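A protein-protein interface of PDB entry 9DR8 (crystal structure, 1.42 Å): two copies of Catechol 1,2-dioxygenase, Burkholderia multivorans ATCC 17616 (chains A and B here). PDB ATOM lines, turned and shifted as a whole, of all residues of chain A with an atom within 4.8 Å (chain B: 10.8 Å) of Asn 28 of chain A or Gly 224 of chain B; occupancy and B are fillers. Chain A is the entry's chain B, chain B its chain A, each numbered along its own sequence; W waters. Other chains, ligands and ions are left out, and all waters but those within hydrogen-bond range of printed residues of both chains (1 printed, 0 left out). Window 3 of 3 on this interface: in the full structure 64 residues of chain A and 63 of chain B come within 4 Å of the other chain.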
ATOM      1  N   LYS A  24      15.924  29.382  -5.035  1.00  0.00           N
ATOM      2  CA  LYS A  24      16.048  28.388  -6.099  1.00  0.00           C
ATOM      3  C   LYS A  24      14.685  27.988  -6.646  1.00  0.00           C
ATOM      4  O   LYS A  24      14.524  27.784  -7.855  1.00  0.00           O
ATOM      5  CB  LYS A  24      16.767  27.146  -5.575  1.00  0.00           C
ATOM      6  CG  LYS A  24      18.247  27.333  -5.331  1.00  0.00           C
ATOM      7  CD  LYS A  24      18.832  26.102  -4.661  1.00  0.00           C
ATOM      8  CE  LYS A  24      20.276  26.314  -4.258  1.00  0.00           C
ATOM      9  NZ  LYS A  24      20.792  25.150  -3.488  1.00  0.00           N
ATOM     10  N   ALA A  25      13.701  27.821  -5.765  1.00  0.00           N
ATOM     11  CA  ALA A  25      12.361  27.482  -6.233  1.00  0.00           C
ATOM     12  C   ALA A  25      11.749  28.629  -7.027  1.00  0.00           C
ATOM     13  O   ALA A  25      11.158  28.413  -8.089  1.00  0.00           O
ATOM     14  CB  ALA A  25      11.470  27.127  -5.048  1.00  0.00           C
ATOM     15  N   ALA A  26      11.874  29.857  -6.522  1.00  0.00           N
ATOM     16  CA  ALA A  26      11.215  30.992  -7.158  1.00  0.00           C
ATOM     17  C   ALA A  26      11.746  31.225  -8.566  1.00  0.00           C
ATOM     18  O   ALA A  26      10.984  31.583  -9.470  1.00  0.00           O
ATOM     19  CB  ALA A  26      11.399  32.240  -6.297  1.00  0.00           C
ATOM     20  N   ALA A  27      13.048  31.017  -8.777  1.00  0.00           N
ATOM     21  CA  ALA A  27      13.640  31.153 -10.101  1.00  0.00           C
ATOM     22  C   ALA A  27      13.617  29.849 -10.894  1.00  0.00           C
ATOM     23  O   ALA A  27      14.060  29.834 -12.047  1.00  0.00           O
ATOM     24  CB  ALA A  27      15.077  31.673  -9.989  1.00  0.00           C
ATOM     25  N   ASN A  28      13.096  28.773 -10.304  1.00  0.00           N
ATOM     26  CA  ASN A  28      12.972  27.467 -10.955  1.00  0.00           C
ATOM     27  C   ASN A  28      14.308  26.935 -11.470  1.00  0.00           C
ATOM     28  O   ASN A  28      14.389  26.363 -12.560  1.00  0.00           O
ATOM     29  CB  ASN A  28      11.915  27.473 -12.056  1.00  0.00           C
ATOM     30  CG  ASN A  28      11.398  26.089 -12.360  1.00  0.00           C
ATOM     31  OD1 ASN A  28      11.451  25.206 -11.507  1.00  0.00           O
ATOM     32  ND2 ASN A  28      10.899  25.888 -13.571  1.00  0.00           N
ATOM     33  N   LEU A  29      15.361  27.077 -10.662  1.00  0.00           N
ATOM     34  CA  LEU A  29      16.671  26.593 -11.091  1.00  0.00           C
ATOM     35  C   LEU A  29      16.683  25.081 -11.265  1.00  0.00           C
ATOM     36  O   LEU A  29      17.378  24.558 -12.145  1.00  0.00           O
ATOM     37  CB  LEU A  29      17.743  27.010 -10.088  1.00  0.00           C
ATOM     38  CG  LEU A  29      18.004  28.509  -9.952  1.00  0.00           C
ATOM     39  CD1 LEU A  29      19.304  28.728  -9.186  1.00  0.00           C
ATOM     40  CD2 LEU A  29      18.066  29.204 -11.302  1.00  0.00           C
ATOM     41  N   ASN A  30      15.940  24.360 -10.429  1.00  0.00           N
ATOM     42  CA  ASN A  30      15.873  22.908 -10.506  1.00  0.00           C
ATOM     43  C   ASN A  30      14.696  22.415 -11.343  1.00  0.00           C
ATOM     44  O   ASN A  30      14.311  21.246 -11.230  1.00  0.00           O
ATOM     45  CB  ASN A  30      15.830  22.305  -9.099  1.00  0.00           C
ATOM     46  CG  ASN A  30      17.040  22.694  -8.261  1.00  0.00           C
ATOM     47  OD1 ASN A  30      16.906  23.135  -7.117  1.00  0.00           O
ATOM     48  ND2 ASN A  30      18.231  22.540  -8.833  1.00  0.00           N
ATOM     49  N   GLY A  31      14.127  23.273 -12.189  1.00  0.00           N
ATOM     50  CA  GLY A  31      13.018  22.885 -13.029  1.00  0.00           C
ATOM     51  C   GLY A  31      13.465  22.094 -14.242  1.00  0.00           C
ATOM     52  O   GLY A  31      14.646  21.820 -14.451  1.00  0.00           O
ATOM     53  N   ASP A  32      12.484  21.713 -15.055  1.00  0.00           N
ATOM     54  CA  ASP A  32      12.773  21.020 -16.298  1.00  0.00           C
ATOM     55  C   ASP A  32      13.437  21.980 -17.283  1.00  0.00           C
ATOM     56  O   ASP A  32      13.448  23.198 -17.093  1.00  0.00           O
ATOM     57  CB  ASP A  32      11.490  20.459 -16.909  1.00  0.00           C
ATOM     58  CG  ASP A  32      10.746  19.530 -15.966  1.00  0.00           C
ATOM     59  OD1 ASP A  32      11.390  18.920 -15.084  1.00  0.00           O
ATOM     60  OD2 ASP A  32       9.511  19.404 -16.113  1.00  0.00           O
ATOM     61  N   ARG A  39      16.264  32.359 -16.158  1.00  0.00           N
ATOM     62  CA  ARG A  39      16.242  31.901 -14.773  1.00  0.00           C
ATOM     63  C   ARG A  39      17.470  32.389 -14.018  1.00  0.00           C
ATOM     64  O   ARG A  39      17.376  32.747 -12.840  1.00  0.00           O
ATOM     65  CB  ARG A  39      16.169  30.375 -14.716  1.00  0.00           C
ATOM     66  CG  ARG A  39      14.883  29.777 -15.241  1.00  0.00           C
ATOM     67  CD  ARG A  39      14.996  28.269 -15.298  1.00  0.00           C
ATOM     68  NE  ARG A  39      13.781  27.651 -15.816  1.00  0.00           N
ATOM     69  CZ  ARG A  39      13.655  26.362 -16.097  1.00  0.00           C
ATOM     70  NH1 ARG A  39      14.644  25.504 -15.877  1.00  0.00           N
ATOM     71  NH2 ARG A  39      12.513  25.920 -16.620  1.00  0.00           N
ATOM     72  N   GLY B  85       4.451  35.841  -5.991  1.00  0.00           N
ATOM     73  CA  GLY B  85       4.859  34.733  -6.840  1.00  0.00           C
ATOM     74  C   GLY B  85       6.352  34.484  -6.884  1.00  0.00           C
ATOM     75  O   GLY B  85       6.772  33.369  -7.200  1.00  0.00           O
ATOM     76  N   ILE B  86       7.169  35.503  -6.617  1.00  0.00           N
ATOM     77  CA  ILE B  86       8.624  35.346  -6.599  1.00  0.00           C
ATOM     78  C   ILE B  86       9.144  35.124  -5.189  1.00  0.00           C
ATOM     79  O   ILE B  86      10.360  35.136  -4.962  1.00  0.00           O
ATOM     80  CB  ILE B  86       9.355  36.527  -7.263  1.00  0.00           C
ATOM     81  CG1 ILE B  86       8.930  37.839  -6.595  1.00  0.00           C
ATOM     82  CG2 ILE B  86       9.075  36.543  -8.741  1.00  0.00           C
ATOM     83  CD1 ILE B  86       9.824  38.377  -5.618  1.00  0.00           C
ATOM     84  N   GLY B  87       8.246  34.952  -4.227  1.00  0.00           N
ATOM     85  CA  GLY B  87       8.654  34.579  -2.895  1.00  0.00           C
ATOM     86  C   GLY B  87       9.048  35.731  -2.003  1.00  0.00           C
ATOM     87  O   GLY B  87       9.421  35.502  -0.850  1.00  0.00           O
ATOM     88  N   THR B 216       2.466  38.908 -14.114  1.00  0.00           N
ATOM     89  CA  THR B 216       2.981  37.865 -13.231  1.00  0.00           C
ATOM     90  C   THR B 216       3.064  36.534 -13.965  1.00  0.00           C
ATOM     91  O   THR B 216       4.107  35.875 -13.961  1.00  0.00           O
ATOM     92  CB  THR B 216       2.129  37.752 -11.968  1.00  0.00           C
ATOM     93  OG1 THR B 216       2.061  39.025 -11.318  1.00  0.00           O
ATOM     94  CG2 THR B 216       2.727  36.746 -10.996  1.00  0.00           C
ATOM     95  N   GLN B 217       1.977  36.135 -14.626  1.00  0.00           N
ATOM     96  CA  GLN B 217       1.997  34.881 -15.366  1.00  0.00           C
ATOM     97  C   GLN B 217       2.995  34.912 -16.519  1.00  0.00           C
ATOM     98  O   GLN B 217       3.572  33.877 -16.857  1.00  0.00           O
ATOM     99  CB  GLN B 217       0.594  34.542 -15.866  1.00  0.00           C
ATOM    100  CG  GLN B 217       0.487  33.117 -16.379  1.00  0.00           C
ATOM    101  CD  GLN B 217       0.734  32.088 -15.288  1.00  0.00           C
ATOM    102  OE1 GLN B 217       0.104  32.117 -14.231  1.00  0.00           O
ATOM    103  NE2 GLN B 217       1.670  31.188 -15.534  1.00  0.00           N
ATOM    104  N   GLN B 218       3.215  36.073 -17.139  1.00  0.00           N
ATOM    105  CA  GLN B 218       4.213  36.152 -18.203  1.00  0.00           C
ATOM    106  C   GLN B 218       5.597  35.794 -17.676  1.00  0.00           C
ATOM    107  O   GLN B 218       6.334  35.016 -18.294  1.00  0.00           O
ATOM    108  CB  GLN B 218       4.203  37.556 -18.796  1.00  0.00           C
ATOM    109  CG  GLN B 218       5.209  37.766 -19.905  1.00  0.00           C
ATOM    110  CD  GLN B 218       5.151  39.173 -20.460  1.00  0.00           C
ATOM    111  OE1 GLN B 218       5.795  40.076 -19.947  1.00  0.00           O
ATOM    112  NE2 GLN B 218       4.351  39.368 -21.492  1.00  0.00           N
ATOM    113  N   LEU B 219       5.963  36.350 -16.522  1.00  0.00           N
ATOM    114  CA  LEU B 219       7.250  36.030 -15.922  1.00  0.00           C
ATOM    115  C   LEU B 219       7.307  34.567 -15.506  1.00  0.00           C
ATOM    116  O   LEU B 219       8.305  33.881 -15.760  1.00  0.00           O
ATOM    117  CB  LEU B 219       7.506  36.973 -14.743  1.00  0.00           C
ATOM    118  CG  LEU B 219       8.789  36.778 -13.938  1.00  0.00           C
ATOM    119  CD1 LEU B 219       9.297  38.126 -13.428  1.00  0.00           C
ATOM    120  CD2 LEU B 219       8.536  35.810 -12.771  1.00  0.00           C
ATOM    121  N   LEU B 220       6.235  34.052 -14.899  1.00  0.00           N
ATOM    122  CA  LEU B 220       6.235  32.647 -14.499  1.00  0.00           C
ATOM    123  C   LEU B 220       6.372  31.736 -15.713  1.00  0.00           C
ATOM    124  O   LEU B 220       7.107  30.747 -15.673  1.00  0.00           O
ATOM    125  CB  LEU B 220       4.967  32.314 -13.715  1.00  0.00           C
ATOM    126  CG  LEU B 220       4.825  33.037 -12.372  1.00  0.00           C
ATOM    127  CD1 LEU B 220       3.414  32.855 -11.804  1.00  0.00           C
ATOM    128  CD2 LEU B 220       5.865  32.558 -11.370  1.00  0.00           C
ATOM    129  N   ASN B 221       5.688  32.066 -16.811  1.00  0.00           N
ATOM    130  CA  ASN B 221       5.837  31.270 -18.022  1.00  0.00           C
ATOM    131  C   ASN B 221       7.290  31.255 -18.473  1.00  0.00           C
ATOM    132  O   ASN B 221       7.809  30.214 -18.896  1.00  0.00           O
ATOM    133  CB  ASN B 221       4.957  31.829 -19.144  1.00  0.00           C
ATOM    134  CG  ASN B 221       3.473  31.596 -18.913  1.00  0.00           C
ATOM    135  OD1 ASN B 221       3.075  30.779 -18.088  1.00  0.00           O
ATOM    136  ND2 ASN B 221       2.647  32.307 -19.667  1.00  0.00           N
ATOM    137  N   GLY B 222       7.962  32.410 -18.398  1.00  0.00           N
ATOM    138  CA  GLY B 222       9.360  32.466 -18.787  1.00  0.00           C
ATOM    139  C   GLY B 222      10.246  31.608 -17.909  1.00  0.00           C
ATOM    140  O   GLY B 222      11.249  31.070 -18.376  1.00  0.00           O
ATOM    141  N   LEU B 223       9.880  31.451 -16.637  1.00  0.00           N
ATOM    142  CA  LEU B 223      10.630  30.600 -15.728  1.00  0.00           C
ATOM    143  C   LEU B 223      10.236  29.133 -15.829  1.00  0.00           C
ATOM    144  O   LEU B 223      10.942  28.288 -15.279  1.00  0.00           O
ATOM    145  CB  LEU B 223      10.408  31.061 -14.285  1.00  0.00           C
ATOM    146  CG  LEU B 223      10.904  32.464 -13.930  1.00  0.00           C
ATOM    147  CD1 LEU B 223      10.432  32.854 -12.538  1.00  0.00           C
ATOM    148  CD2 LEU B 223      12.435  32.556 -14.015  1.00  0.00           C
ATOM    149  N   GLY B 224       9.134  28.815 -16.508  1.00  0.00           N
ATOM    150  CA  GLY B 224       8.636  27.456 -16.541  1.00  0.00           C
ATOM    151  C   GLY B 224       7.807  27.063 -15.340  1.00  0.00           C
ATOM    152  O   GLY B 224       7.706  25.874 -15.038  1.00  0.00           O
ATOM    153  N   ARG B 225       7.213  28.028 -14.645  1.00  0.00           N
ATOM    154  CA  ARG B 225       6.480  27.789 -13.413  1.00  0.00           C
ATOM    155  C   ARG B 225       4.991  28.028 -13.621  1.00  0.00           C
ATOM    156  O   ARG B 225       4.595  28.873 -14.420  1.00  0.00           O
ATOM    157  CB  ARG B 225       6.950  28.759 -12.320  1.00  0.00           C
ATOM    158  CG  ARG B 225       8.329  28.446 -11.747  1.00  0.00           C
ATOM    159  CD  ARG B 225       8.712  29.429 -10.661  1.00  0.00           C
ATOM    160  NE  ARG B 225       7.674  29.477  -9.638  1.00  0.00           N
ATOM    161  CZ  ARG B 225       7.390  30.530  -8.885  1.00  0.00           C
ATOM    162  NH1 ARG B 225       8.156  31.614  -8.885  1.00  0.00           N
ATOM    163  NH2 ARG B 225       6.287  30.515  -8.148  1.00  0.00           N
ATOM    164  N   HIS B 226       4.166  27.305 -12.865  1.00  0.00           N
ATOM    165  CA  HIS B 226       2.742  27.596 -12.824  1.00  0.00           C
ATOM    166  C   HIS B 226       2.460  28.744 -11.856  1.00  0.00           C
ATOM    167  O   HIS B 226       3.281  29.086 -10.996  1.00  0.00           O
ATOM    168  CB  HIS B 226       1.932  26.354 -12.418  1.00  0.00           C
ATOM    169  CG  HIS B 226       2.022  26.008 -10.963  1.00  0.00           C
ATOM    170  ND1 HIS B 226       1.350  26.711  -9.988  1.00  0.00           N
ATOM    171  CD2 HIS B 226       2.704  25.034 -10.318  1.00  0.00           C
ATOM    172  CE1 HIS B 226       1.608  26.182  -8.805  1.00  0.00           C
ATOM    173  NE2 HIS B 226       2.433  25.167  -8.980  1.00  0.00           N
ATOM    174  N   GLY B 227       1.272  29.340 -12.010  1.00  0.00           N
ATOM    175  CA  GLY B 227       0.851  30.458 -11.186  1.00  0.00           C
ATOM    176  C   GLY B 227      -0.404  30.185 -10.376  1.00  0.00           C
ATOM    177  O   GLY B 227      -1.233  31.076 -10.181  1.00  0.00           O
ATOM    178  N   ASN B 228      -0.528  28.972  -9.849  1.00  0.00           N
ATOM    179  CA  ASN B 228      -1.735  28.525  -9.175  1.00  0.00           C
ATOM    180  C   ASN B 228      -1.533  28.429  -7.669  1.00  0.00           C
ATOM    181  O   ASN B 228      -0.432  28.163  -7.181  1.00  0.00           O
ATOM    182  CB  ASN B 228      -2.152  27.147  -9.702  1.00  0.00           C
ATOM    183  CG  ASN B 228      -2.488  27.174 -11.175  1.00  0.00           C
ATOM    184  OD1 ASN B 228      -3.204  28.054 -11.641  1.00  0.00           O
ATOM    185  ND2 ASN B 228      -1.947  26.222 -11.921  1.00  0.00           N
ATOM    186  N   ASP B 259       2.363  22.963  -3.293  1.00  0.00           N
ATOM    187  CA  ASP B 259       2.947  23.516  -4.507  1.00  0.00           C
ATOM    188  C   ASP B 259       2.310  24.861  -4.836  1.00  0.00           C
ATOM    189  O   ASP B 259       2.042  25.183  -5.998  1.00  0.00           O
ATOM    190  CB  ASP B 259       2.828  22.539  -5.676  1.00  0.00           C
ATOM    191  CG  ASP B 259       3.756  22.898  -6.830  1.00  0.00           C
ATOM    192  OD1 ASP B 259       4.752  23.615  -6.599  1.00  0.00           O
ATOM    193  OD2 ASP B 259       3.490  22.466  -7.966  1.00  0.00           O
ATOM    194  N   PHE B 261       2.177  28.600  -5.687  1.00  0.00           N
ATOM    195  CA  PHE B 261       3.120  29.476  -6.378  1.00  0.00           C
ATOM    196  C   PHE B 261       3.595  30.629  -5.499  1.00  0.00           C
ATOM    197  O   PHE B 261       4.576  31.284  -5.849  1.00  0.00           O
ATOM    198  CB  PHE B 261       2.525  29.977  -7.712  1.00  0.00           C
ATOM    199  CG  PHE B 261       1.876  31.337  -7.642  1.00  0.00           C
ATOM    200  CD1 PHE B 261       0.660  31.519  -7.029  1.00  0.00           C
ATOM    201  CD2 PHE B 261       2.494  32.435  -8.217  1.00  0.00           C
ATOM    202  CE1 PHE B 261       0.070  32.777  -6.984  1.00  0.00           C
ATOM    203  CE2 PHE B 261       1.915  33.682  -8.173  1.00  0.00           C
ATOM    204  CZ  PHE B 261       0.705  33.855  -7.552  1.00  0.00           C
ATOM    205  N   TYR B 263       4.093  30.087  -2.051  1.00  0.00           N
ATOM    206  CA  TYR B 263       4.926  29.506  -0.994  1.00  0.00           C
ATOM    207  C   TYR B 263       4.337  29.691   0.405  1.00  0.00           C
ATOM    208  O   TYR B 263       5.078  29.782   1.388  1.00  0.00           O
ATOM    209  CB  TYR B 263       6.354  30.062  -1.072  1.00  0.00           C
ATOM    210  CG  TYR B 263       6.943  29.854  -2.449  1.00  0.00           C
ATOM    211  CD1 TYR B 263       7.321  28.593  -2.878  1.00  0.00           C
ATOM    212  CD2 TYR B 263       7.101  30.913  -3.330  1.00  0.00           C
ATOM    213  CE1 TYR B 263       7.844  28.394  -4.132  1.00  0.00           C
ATOM    214  CE2 TYR B 263       7.617  30.719  -4.592  1.00  0.00           C
ATOM    215  CZ  TYR B 263       7.997  29.464  -4.986  1.00  0.00           C
ATOM    216  OH  TYR B 263       8.515  29.281  -6.246  1.00  0.00           O
HETATM  217  O   HOH W   1      11.955  28.329 -18.366  1.00  0.00           O
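No position is printed for both chains. Of the 11 pairs that touch across the chains among the printed residues, none has its exchanged pair printed and touching as well.
The side-chain amide oxygen of Asn 28 of chain A sits close to the backbone NH of Gly 31 of chain A, at 3.4 Å. NH1 of Arg 39 of chain A sits close to O of Asn 28 of chain A (3.4 Å). O of Phe 261 of chain B lies within hydrogen-bond range of NH2 of Arg 225 of chain B (3.0 Å). The backbone carbonyl oxygen (O) of Leu 220 of chain B sits at hydrogen-bond distance from the backbone NH (N) of Arg 225 of chain B (2.9 Å). The backbone carbonyl oxygen (O) of Gly 85 of chain B lies within hydrogen-bond range of the guanidinium group (NH1) of Arg 225 of chain B (2.8 Å). The guanidinium group (NH1) of Arg 39 of chain A sits at hydrogen-bond distance from the backbone carbonyl oxygen (O) of Asp 32 of chain A.
Of the 19 printed residues of chain B, 5 touch a printed residue of chain A. Printed residues of chain B that touch a printed residue of chain A: Ile 86, Leu 223, Gly 224, Arg 225 and Tyr 263. Hydrophobic or aromatic side chains of chain A within 4 Å of the printed part of chain B: Ala 25 and Ala 26. Among the printed residues, 11 pairs touch across the chains. Among the printed residues, no Asp or Glu carboxylate lies within 4 Å of a Lys or Arg side-chain nitrogen of the other chain.
Of the printed residues of chain B, Asn 28 of chain A touches Leu 223, Gly 224 and Arg 225. Printed residues of chain A within 4 Å of Gly 224 of chain B: Asn 28. Ala 25 of chain A touches just these residues of chain B: Arg 225 (3.7 Å) and Tyr 263 (3.3 Å). Ala 27 of chain A touches just one residue of chain B: Leu 223. No residue of chain B comes within 4 Å of Leu 29 of chain A. Asn 30 of chain A touches none of the printed residues of chain B. Of the printed residues of chain A, Ile 86 of chain B touches Ala 26 (3.4 Å). Of the printed residues of chain B, Arg 39 of chain A touches Leu 223 (3.0 Å). Gly 85 of chain B touches none of the printed residues of chain A. Gly 222 of chain B touches none of the printed residues of chain A. The nearest residue of chain A that does not touch Gly 224 of chain B is Arg 39 of chain A (4.2 Å).
CD of Arg 225 of chain B touches O of Ala 25 of chain A (3.7 Å). Ala 26 of chain A touches Ile 86 of chain B. O of Ala 26 of chain A touches CD1 of Leu 223 of chain B (3.4 Å). Ala 27 of chain A touches Leu 223 of chain B (O to CD2, 3.7 Å). ND2 of Asn 28 of chain A touches O of Gly 224 of chain B, at 3.5 Å. Asn 28 of chain A touches Arg 225 of chain B.
Water W1 lies within hydrogen-bond range of O of Gly 222 of chain B (2.8 Å), NH2 of Arg 39 of chain A (3.0 Å), O of Leu 223 of chain B (3.2 Å) and N of Gly 224 of chain B (3.4 Å).
OH of Tyr 263 of chain B sits close to N of Ala 26 of chain A, at 3.4 Å. The side-chain amide nitrogen (ND2) of Asn 28 of chain A is in hydrogen-bond range of the backbone carbonyl oxygen (O) of Leu 223 of chain B (2.9 Å). O of Leu 223 of chain B is in hydrogen-bond range of NE of Arg 39 of chain A (3.0 Å). The backbone carbonyl oxygen of Ala 26 of chain A sits at hydrogen-bond distance from the guanidinium group of Arg 225 of chain B (2.9 Å). O of Ala 25 of chain A is in hydrogen-bond range of OH of Tyr 263 of chain B, 3.3 Å away.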
